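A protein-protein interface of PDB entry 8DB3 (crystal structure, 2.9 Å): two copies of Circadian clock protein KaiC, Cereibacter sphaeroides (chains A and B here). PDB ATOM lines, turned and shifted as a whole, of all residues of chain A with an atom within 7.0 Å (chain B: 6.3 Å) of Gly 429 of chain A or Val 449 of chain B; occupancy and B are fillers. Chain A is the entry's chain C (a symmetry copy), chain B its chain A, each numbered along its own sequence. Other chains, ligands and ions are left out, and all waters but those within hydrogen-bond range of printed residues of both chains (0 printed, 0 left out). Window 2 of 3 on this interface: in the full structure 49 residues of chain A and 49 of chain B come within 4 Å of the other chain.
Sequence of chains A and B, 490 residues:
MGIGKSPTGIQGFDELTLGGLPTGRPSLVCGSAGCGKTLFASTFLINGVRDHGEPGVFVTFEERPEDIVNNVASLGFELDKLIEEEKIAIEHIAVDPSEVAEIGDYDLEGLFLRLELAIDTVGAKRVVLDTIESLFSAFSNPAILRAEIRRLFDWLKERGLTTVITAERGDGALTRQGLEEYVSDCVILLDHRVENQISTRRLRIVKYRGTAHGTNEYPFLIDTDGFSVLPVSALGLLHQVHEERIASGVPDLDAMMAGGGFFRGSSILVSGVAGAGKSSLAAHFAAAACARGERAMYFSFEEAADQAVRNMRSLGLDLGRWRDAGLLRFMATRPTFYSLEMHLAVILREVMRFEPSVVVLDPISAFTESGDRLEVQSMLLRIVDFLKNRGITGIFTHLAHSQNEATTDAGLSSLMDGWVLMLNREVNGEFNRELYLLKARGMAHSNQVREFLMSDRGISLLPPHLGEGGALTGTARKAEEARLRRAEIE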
ATOM      1  N   GLU A 426      14.112  25.505   3.555  1.00  0.00           N
ATOM      2  CA  GLU A 426      13.917  25.333   4.988  1.00  0.00           C
ATOM      3  C   GLU A 426      13.645  23.871   5.309  1.00  0.00           C
ATOM      4  O   GLU A 426      12.850  23.213   4.630  1.00  0.00           O
ATOM      5  CB  GLU A 426      12.755  26.197   5.477  1.00  0.00           C
ATOM      6  CG  GLU A 426      12.621  26.265   6.993  1.00  0.00           C
ATOM      7  CD  GLU A 426      11.182  26.144   7.461  1.00  0.00           C
ATOM      8  OE1 GLU A 426      10.283  26.648   6.755  1.00  0.00           O
ATOM      9  OE2 GLU A 426      10.952  25.546   8.534  1.00  0.00           O
ATOM     10  N   VAL A 427      14.308  23.365   6.345  1.00  0.00           N
ATOM     11  CA  VAL A 427      14.051  22.024   6.860  1.00  0.00           C
ATOM     12  C   VAL A 427      14.352  22.030   8.353  1.00  0.00           C
ATOM     13  O   VAL A 427      15.412  22.500   8.780  1.00  0.00           O
ATOM     14  CB  VAL A 427      14.885  20.945   6.141  1.00  0.00           C
ATOM     15  CG1 VAL A 427      14.634  20.972   4.637  1.00  0.00           C
ATOM     16  CG2 VAL A 427      16.361  21.124   6.445  1.00  0.00           C
ATOM     17  N   ASN A 428      13.412  21.508   9.146  1.00  0.00           N
ATOM     18  CA  ASN A 428      13.581  21.423  10.597  1.00  0.00           C
ATOM     19  C   ASN A 428      13.966  22.779  11.176  1.00  0.00           C
ATOM     20  O   ASN A 428      14.866  22.892  12.014  1.00  0.00           O
ATOM     21  CB  ASN A 428      14.607  20.351  10.963  1.00  0.00           C
ATOM     22  CG  ASN A 428      14.646  20.061  12.451  1.00  0.00           C
ATOM     23  OD1 ASN A 428      14.020  20.758  13.249  1.00  0.00           O
ATOM     24  ND2 ASN A 428      15.388  19.028  12.830  1.00  0.00           N
ATOM     25  N   GLY A 429      13.283  23.825  10.724  1.00  0.00           N
ATOM     26  CA  GLY A 429      13.553  25.163  11.196  1.00  0.00           C
ATOM     27  C   GLY A 429      14.976  25.606  10.938  1.00  0.00           C
ATOM     28  O   GLY A 429      15.659  26.088  11.846  1.00  0.00           O
ATOM     29  N   GLU A 430      15.433  25.451   9.699  1.00  0.00           N
ATOM     30  CA  GLU A 430      16.765  25.892   9.310  1.00  0.00           C
ATOM     31  C   GLU A 430      16.873  25.829   7.795  1.00  0.00           C
ATOM     32  O   GLU A 430      16.289  24.950   7.155  1.00  0.00           O
ATOM     33  CB  GLU A 430      17.856  25.034   9.959  1.00  0.00           C
ATOM     34  CG  GLU A 430      19.124  25.804  10.298  1.00  0.00           C
ATOM     35  CD  GLU A 430      20.220  24.911  10.845  1.00  0.00           C
ATOM     36  OE1 GLU A 430      20.112  23.674  10.696  1.00  0.00           O
ATOM     37  OE2 GLU A 430      21.190  25.448  11.423  1.00  0.00           O
ATOM     38  N   PHE A 431      17.628  26.770   7.234  1.00  0.00           N
ATOM     39  CA  PHE A 431      17.795  26.888   5.792  1.00  0.00           C
ATOM     40  C   PHE A 431      19.112  26.243   5.382  1.00  0.00           C
ATOM     41  O   PHE A 431      20.180  26.642   5.863  1.00  0.00           O
ATOM     42  CB  PHE A 431      17.761  28.354   5.359  1.00  0.00           C
ATOM     43  CG  PHE A 431      16.399  28.981   5.449  1.00  0.00           C
ATOM     44  CD1 PHE A 431      16.109  29.900   6.442  1.00  0.00           C
ATOM     45  CD2 PHE A 431      15.410  28.650   4.538  1.00  0.00           C
ATOM     46  CE1 PHE A 431      14.856  30.477   6.526  1.00  0.00           C
ATOM     47  CE2 PHE A 431      14.159  29.229   4.614  1.00  0.00           C
ATOM     48  CZ  PHE A 431      13.879  30.137   5.613  1.00  0.00           C
ATOM     49  N   MET B 256      21.562  38.474  14.859  1.00  0.00           N
ATOM     50  CA  MET B 256      21.635  37.360  13.921  1.00  0.00           C
ATOM     51  C   MET B 256      22.612  37.630  12.779  1.00  0.00           C
ATOM     52  O   MET B 256      23.128  36.682  12.175  1.00  0.00           O
ATOM     53  CB  MET B 256      20.248  37.059  13.340  1.00  0.00           C
ATOM     54  CG  MET B 256      19.419  36.090  14.167  1.00  0.00           C
ATOM     55  SD  MET B 256      17.787  35.722  13.478  1.00  0.00           S
ATOM     56  CE  MET B 256      17.537  37.077  12.338  1.00  0.00           C
ATOM     57  N   ARG B 425       2.041  31.159  11.315  1.00  0.00           N
ATOM     58  CA  ARG B 425       1.608  29.922  10.680  1.00  0.00           C
ATOM     59  C   ARG B 425       0.775  29.069  11.626  1.00  0.00           C
ATOM     60  O   ARG B 425       1.074  28.968  12.816  1.00  0.00           O
ATOM     61  CB  ARG B 425       2.816  29.120  10.189  1.00  0.00           C
ATOM     62  CG  ARG B 425       3.383  29.616   8.870  1.00  0.00           C
ATOM     63  CD  ARG B 425       4.382  28.630   8.295  1.00  0.00           C
ATOM     64  NE  ARG B 425       5.517  28.428   9.187  1.00  0.00           N
ATOM     65  CZ  ARG B 425       6.622  27.774   8.860  1.00  0.00           C
ATOM     66  NH1 ARG B 425       6.784  27.248   7.657  1.00  0.00           N
ATOM     67  NH2 ARG B 425       7.590  27.642   9.763  1.00  0.00           N
ATOM     68  N   GLU B 434       7.035  33.162  13.777  1.00  0.00           N
ATOM     69  CA  GLU B 434       8.429  32.859  13.485  1.00  0.00           C
ATOM     70  C   GLU B 434       9.020  33.922  12.566  1.00  0.00           C
ATOM     71  O   GLU B 434       8.304  34.717  11.949  1.00  0.00           O
ATOM     72  CB  GLU B 434       8.568  31.470  12.841  1.00  0.00           C
ATOM     73  CG  GLU B 434       7.642  30.415  13.428  1.00  0.00           C
ATOM     74  CD  GLU B 434       7.779  29.070  12.742  1.00  0.00           C
ATOM     75  OE1 GLU B 434       8.916  28.559  12.656  1.00  0.00           O
ATOM     76  OE2 GLU B 434       6.753  28.523  12.288  1.00  0.00           O
ATOM     77  N   LEU B 435      10.351  33.915  12.471  1.00  0.00           N
ATOM     78  CA  LEU B 435      11.079  34.871  11.652  1.00  0.00           C
ATOM     79  C   LEU B 435      12.197  34.167  10.899  1.00  0.00           C
ATOM     80  O   LEU B 435      12.926  33.347  11.477  1.00  0.00           O
ATOM     81  CB  LEU B 435      11.665  35.998  12.512  1.00  0.00           C
ATOM     82  CG  LEU B 435      12.032  37.286  11.778  1.00  0.00           C
ATOM     83  CD1 LEU B 435      10.787  37.934  11.197  1.00  0.00           C
ATOM     84  CD2 LEU B 435      12.759  38.251  12.699  1.00  0.00           C
ATOM     85  N   TYR B 436      12.309  34.492   9.605  1.00  0.00           N
ATOM     86  CA  TYR B 436      13.416  34.086   8.759  1.00  0.00           C
ATOM     87  C   TYR B 436      14.186  35.322   8.303  1.00  0.00           C
ATOM     88  O   TYR B 436      13.581  36.338   7.936  1.00  0.00           O
ATOM     89  CB  TYR B 436      12.957  33.347   7.491  1.00  0.00           C
ATOM     90  CG  TYR B 436      12.034  32.172   7.681  1.00  0.00           C
ATOM     91  CD1 TYR B 436      12.337  31.155   8.569  1.00  0.00           C
ATOM     92  CD2 TYR B 436      10.867  32.063   6.937  1.00  0.00           C
ATOM     93  CE1 TYR B 436      11.492  30.070   8.726  1.00  0.00           C
ATOM     94  CE2 TYR B 436      10.020  30.985   7.088  1.00  0.00           C
ATOM     95  CZ  TYR B 436      10.335  29.990   7.986  1.00  0.00           C
ATOM     96  OH  TYR B 436       9.497  28.909   8.146  1.00  0.00           O
ATOM     97  N   SER B 446      22.319  34.220  10.349  1.00  0.00           N
ATOM     98  CA  SER B 446      21.878  32.940  10.881  1.00  0.00           C
ATOM     99  C   SER B 446      20.961  32.260   9.871  1.00  0.00           C
ATOM    100  O   SER B 446      19.943  32.831   9.464  1.00  0.00           O
ATOM    101  CB  SER B 446      21.156  33.136  12.212  1.00  0.00           C
ATOM    102  OG  SER B 446      20.757  31.893  12.755  1.00  0.00           O
ATOM    103  N   ASN B 447      21.327  31.044   9.461  1.00  0.00           N
ATOM    104  CA  ASN B 447      20.423  30.219   8.675  1.00  0.00           C
ATOM    105  C   ASN B 447      19.272  29.672   9.506  1.00  0.00           C
ATOM    106  O   ASN B 447      18.394  29.000   8.952  1.00  0.00           O
ATOM    107  CB  ASN B 447      21.188  29.056   8.041  1.00  0.00           C
ATOM    108  CG  ASN B 447      22.179  28.418   8.995  1.00  0.00           C
ATOM    109  OD1 ASN B 447      23.096  29.079   9.482  1.00  0.00           O
ATOM    110  ND2 ASN B 447      21.996  27.132   9.272  1.00  0.00           N
ATOM    111  N   GLN B 448      19.254  29.942  10.807  1.00  0.00           N
ATOM    112  CA  GLN B 448      18.262  29.373  11.703  1.00  0.00           C
ATOM    113  C   GLN B 448      16.998  30.221  11.726  1.00  0.00           C
ATOM    114  O   GLN B 448      17.036  31.442  11.550  1.00  0.00           O
ATOM    115  CB  GLN B 448      18.817  29.253  13.124  1.00  0.00           C
ATOM    116  CG  GLN B 448      20.290  28.893  13.197  1.00  0.00           C
ATOM    117  CD  GLN B 448      20.574  27.820  14.230  1.00  0.00           C
ATOM    118  OE1 GLN B 448      19.858  26.820  14.315  1.00  0.00           O
ATOM    119  NE2 GLN B 448      21.620  28.021  15.022  1.00  0.00           N
ATOM    120  N   VAL B 449      15.876  29.550  11.940  1.00  0.00           N
ATOM    121  CA  VAL B 449      14.595  30.213  12.149  1.00  0.00           C
ATOM    122  C   VAL B 449      14.502  30.631  13.607  1.00  0.00           C
ATOM    123  O   VAL B 449      14.977  29.918  14.497  1.00  0.00           O
ATOM    124  CB  VAL B 449      13.437  29.275  11.765  1.00  0.00           C
ATOM    125  CG1 VAL B 449      12.116  30.028  11.795  1.00  0.00           C
ATOM    126  CG2 VAL B 449      13.718  28.638  10.409  1.00  0.00           C
ATOM    127  N   ARG B 450      13.884  31.781  13.868  1.00  0.00           N
ATOM    128  CA  ARG B 450      13.792  32.280  15.236  1.00  0.00           C
ATOM    129  C   ARG B 450      12.343  32.571  15.582  1.00  0.00           C
ATOM    130  O   ARG B 450      11.709  33.422  14.953  1.00  0.00           O
ATOM    131  CB  ARG B 450      14.667  33.523  15.417  1.00  0.00           C
ATOM    132  CG  ARG B 450      16.140  33.233  15.169  1.00  0.00           C
ATOM    133  CD  ARG B 450      17.045  34.093  16.026  1.00  0.00           C
ATOM    134  NE  ARG B 450      17.106  33.656  17.415  1.00  0.00           N
ATOM    135  CZ  ARG B 450      17.639  34.373  18.394  1.00  0.00           C
ATOM    136  NH1 ARG B 450      18.160  35.568  18.169  1.00  0.00           N
ATOM    137  NH2 ARG B 450      17.651  33.879  19.629  1.00  0.00           N
ATOM    138  N   GLU B 451      11.816  31.851  16.568  1.00  0.00           N
ATOM    139  CA  GLU B 451      10.468  32.121  17.045  1.00  0.00           C
ATOM    140  C   GLU B 451      10.457  33.435  17.814  1.00  0.00           C
ATOM    141  O   GLU B 451      11.286  33.656  18.707  1.00  0.00           O
ATOM    142  CB  GLU B 451       9.972  30.982  17.927  1.00  0.00           C
ATOM    143  CG  GLU B 451       9.817  29.665  17.192  1.00  0.00           C
ATOM    144  CD  GLU B 451       9.517  28.515  18.126  1.00  0.00           C
ATOM    145  OE1 GLU B 451       9.258  28.775  19.321  1.00  0.00           O
ATOM    146  OE2 GLU B 451       9.542  27.352  17.669  1.00  0.00           O
ATOM    147  N   LEU B 462      13.702  34.169  20.357  1.00  0.00           N
ATOM    148  CA  LEU B 462      14.415  33.154  21.120  1.00  0.00           C
ATOM    149  C   LEU B 462      14.989  32.133  20.154  1.00  0.00           C
ATOM    150  O   LEU B 462      14.558  32.054  18.998  1.00  0.00           O
ATOM    151  CB  LEU B 462      13.504  32.475  22.148  1.00  0.00           C
ATOM    152  CG  LEU B 462      12.501  31.443  21.636  1.00  0.00           C
ATOM    153  CD1 LEU B 462      13.115  30.051  21.564  1.00  0.00           C
ATOM    154  CD2 LEU B 462      11.258  31.446  22.528  1.00  0.00           C
ATOM    155  N   PRO B 463      15.972  31.327  20.598  1.00  0.00           N
ATOM    156  CA  PRO B 463      16.655  30.362  19.728  1.00  0.00           C
ATOM    157  C   PRO B 463      15.989  28.992  19.688  1.00  0.00           C
ATOM    158  O   PRO B 463      16.634  28.024  19.280  1.00  0.00           O
ATOM    159  CB  PRO B 463      18.050  30.265  20.359  1.00  0.00           C
ATOM    160  CG  PRO B 463      17.791  30.470  21.832  1.00  0.00           C
ATOM    161  CD  PRO B 463      16.538  31.333  21.962  1.00  0.00           C
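O of Asn 447 of chain B lies within hydrogen-bond range of N of Phe 431 of chain A, 2.9 Å away.
The side-chain amide nitrogen (ND2) of Asn 447 of chain B is in hydrogen-bond range of the side-chain carboxylate (OE2) of Glu 430 of chain A (2.8 Å).
OE1 of Glu 426 of chain A is in salt-bridge range of NH1 of Arg 425 of chain B, at 3.7 Å.
The backbone NH (N) of Val 449 of chain B lies within hydrogen-bond range of the backbone carbonyl oxygen (O) of Gly 429 of chain A, at 3.5 Å.
OE2 of Glu 430 of chain A lies close to OE1 of Gln 448 of chain B.
The side-chain hydroxyl (OH) of Tyr 436 of chain B sits at hydrogen-bond distance from the side-chain carboxylate (OE1) of Glu 426 of chain A (2.8 Å).
NH2 of Arg 425 of chain B lies within salt-bridge range of OE2 of Glu 434 of chain B (2.8 Å).
The backbone NH of Gln 448 of chain B lies close to the side-chain hydroxyl of Ser 446 of chain B, 3.1 Å away.
The guanidinium group of Arg 425 of chain B sits at hydrogen-bond distance from the side-chain hydroxyl of Tyr 436 of chain B, at 2.8 Å.
Glu 430 of chain A touches Val 449 of chain B.
CE1 of Phe 431 of chain A touches CD1 of Tyr 436 of chain B (3.3 Å).
Gly 429 of chain A touches just one residue of chain B: Val 449.
Of chain A, only Gly 429 and Glu 430 come within 4 Å of Val 449 of chain B.
Printed residues of chain B within 4 Å of Phe 431 of chain A: Tyr 436 (3.3 Å) and Asn 447 (2.9 Å).
Of the printed residues of chain A, Arg 425 of chain B touches Glu 426 (3.7 Å).
Printed residues of chain B within 4 Å of Glu 426 of chain A: Arg 425 (3.7 Å) and Tyr 436 (2.8 Å).
Printed residues of chain A within 4 Å of Gln 448 of chain B: Glu 430.
Printed residues of chain A within 4 Å of Asn 447 of chain B: Glu 430 and Phe 431.
Met 256 of chain B touches none of the printed residues of chain A.
Glu 434 of chain B touches none of the printed residues of chain A.
Of the 6 printed residues of chain A, 4 touch a printed residue of chain B.
Hydrophobic or aromatic side chains of chain B that line the printed part of chain A: Tyr 436 and Val 449.
Among the printed residues, Asp or Glu carboxylates within 4 Å of a Lys or Arg side-chain nitrogen of the other chain: Glu 426 of chain A with Arg 425 of chain B (3.7 Å).
No position is printed for both chains.
Of the 8 pairs that touch across the chains among the printed residues, none has its exchanged pair printed and touching as well.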
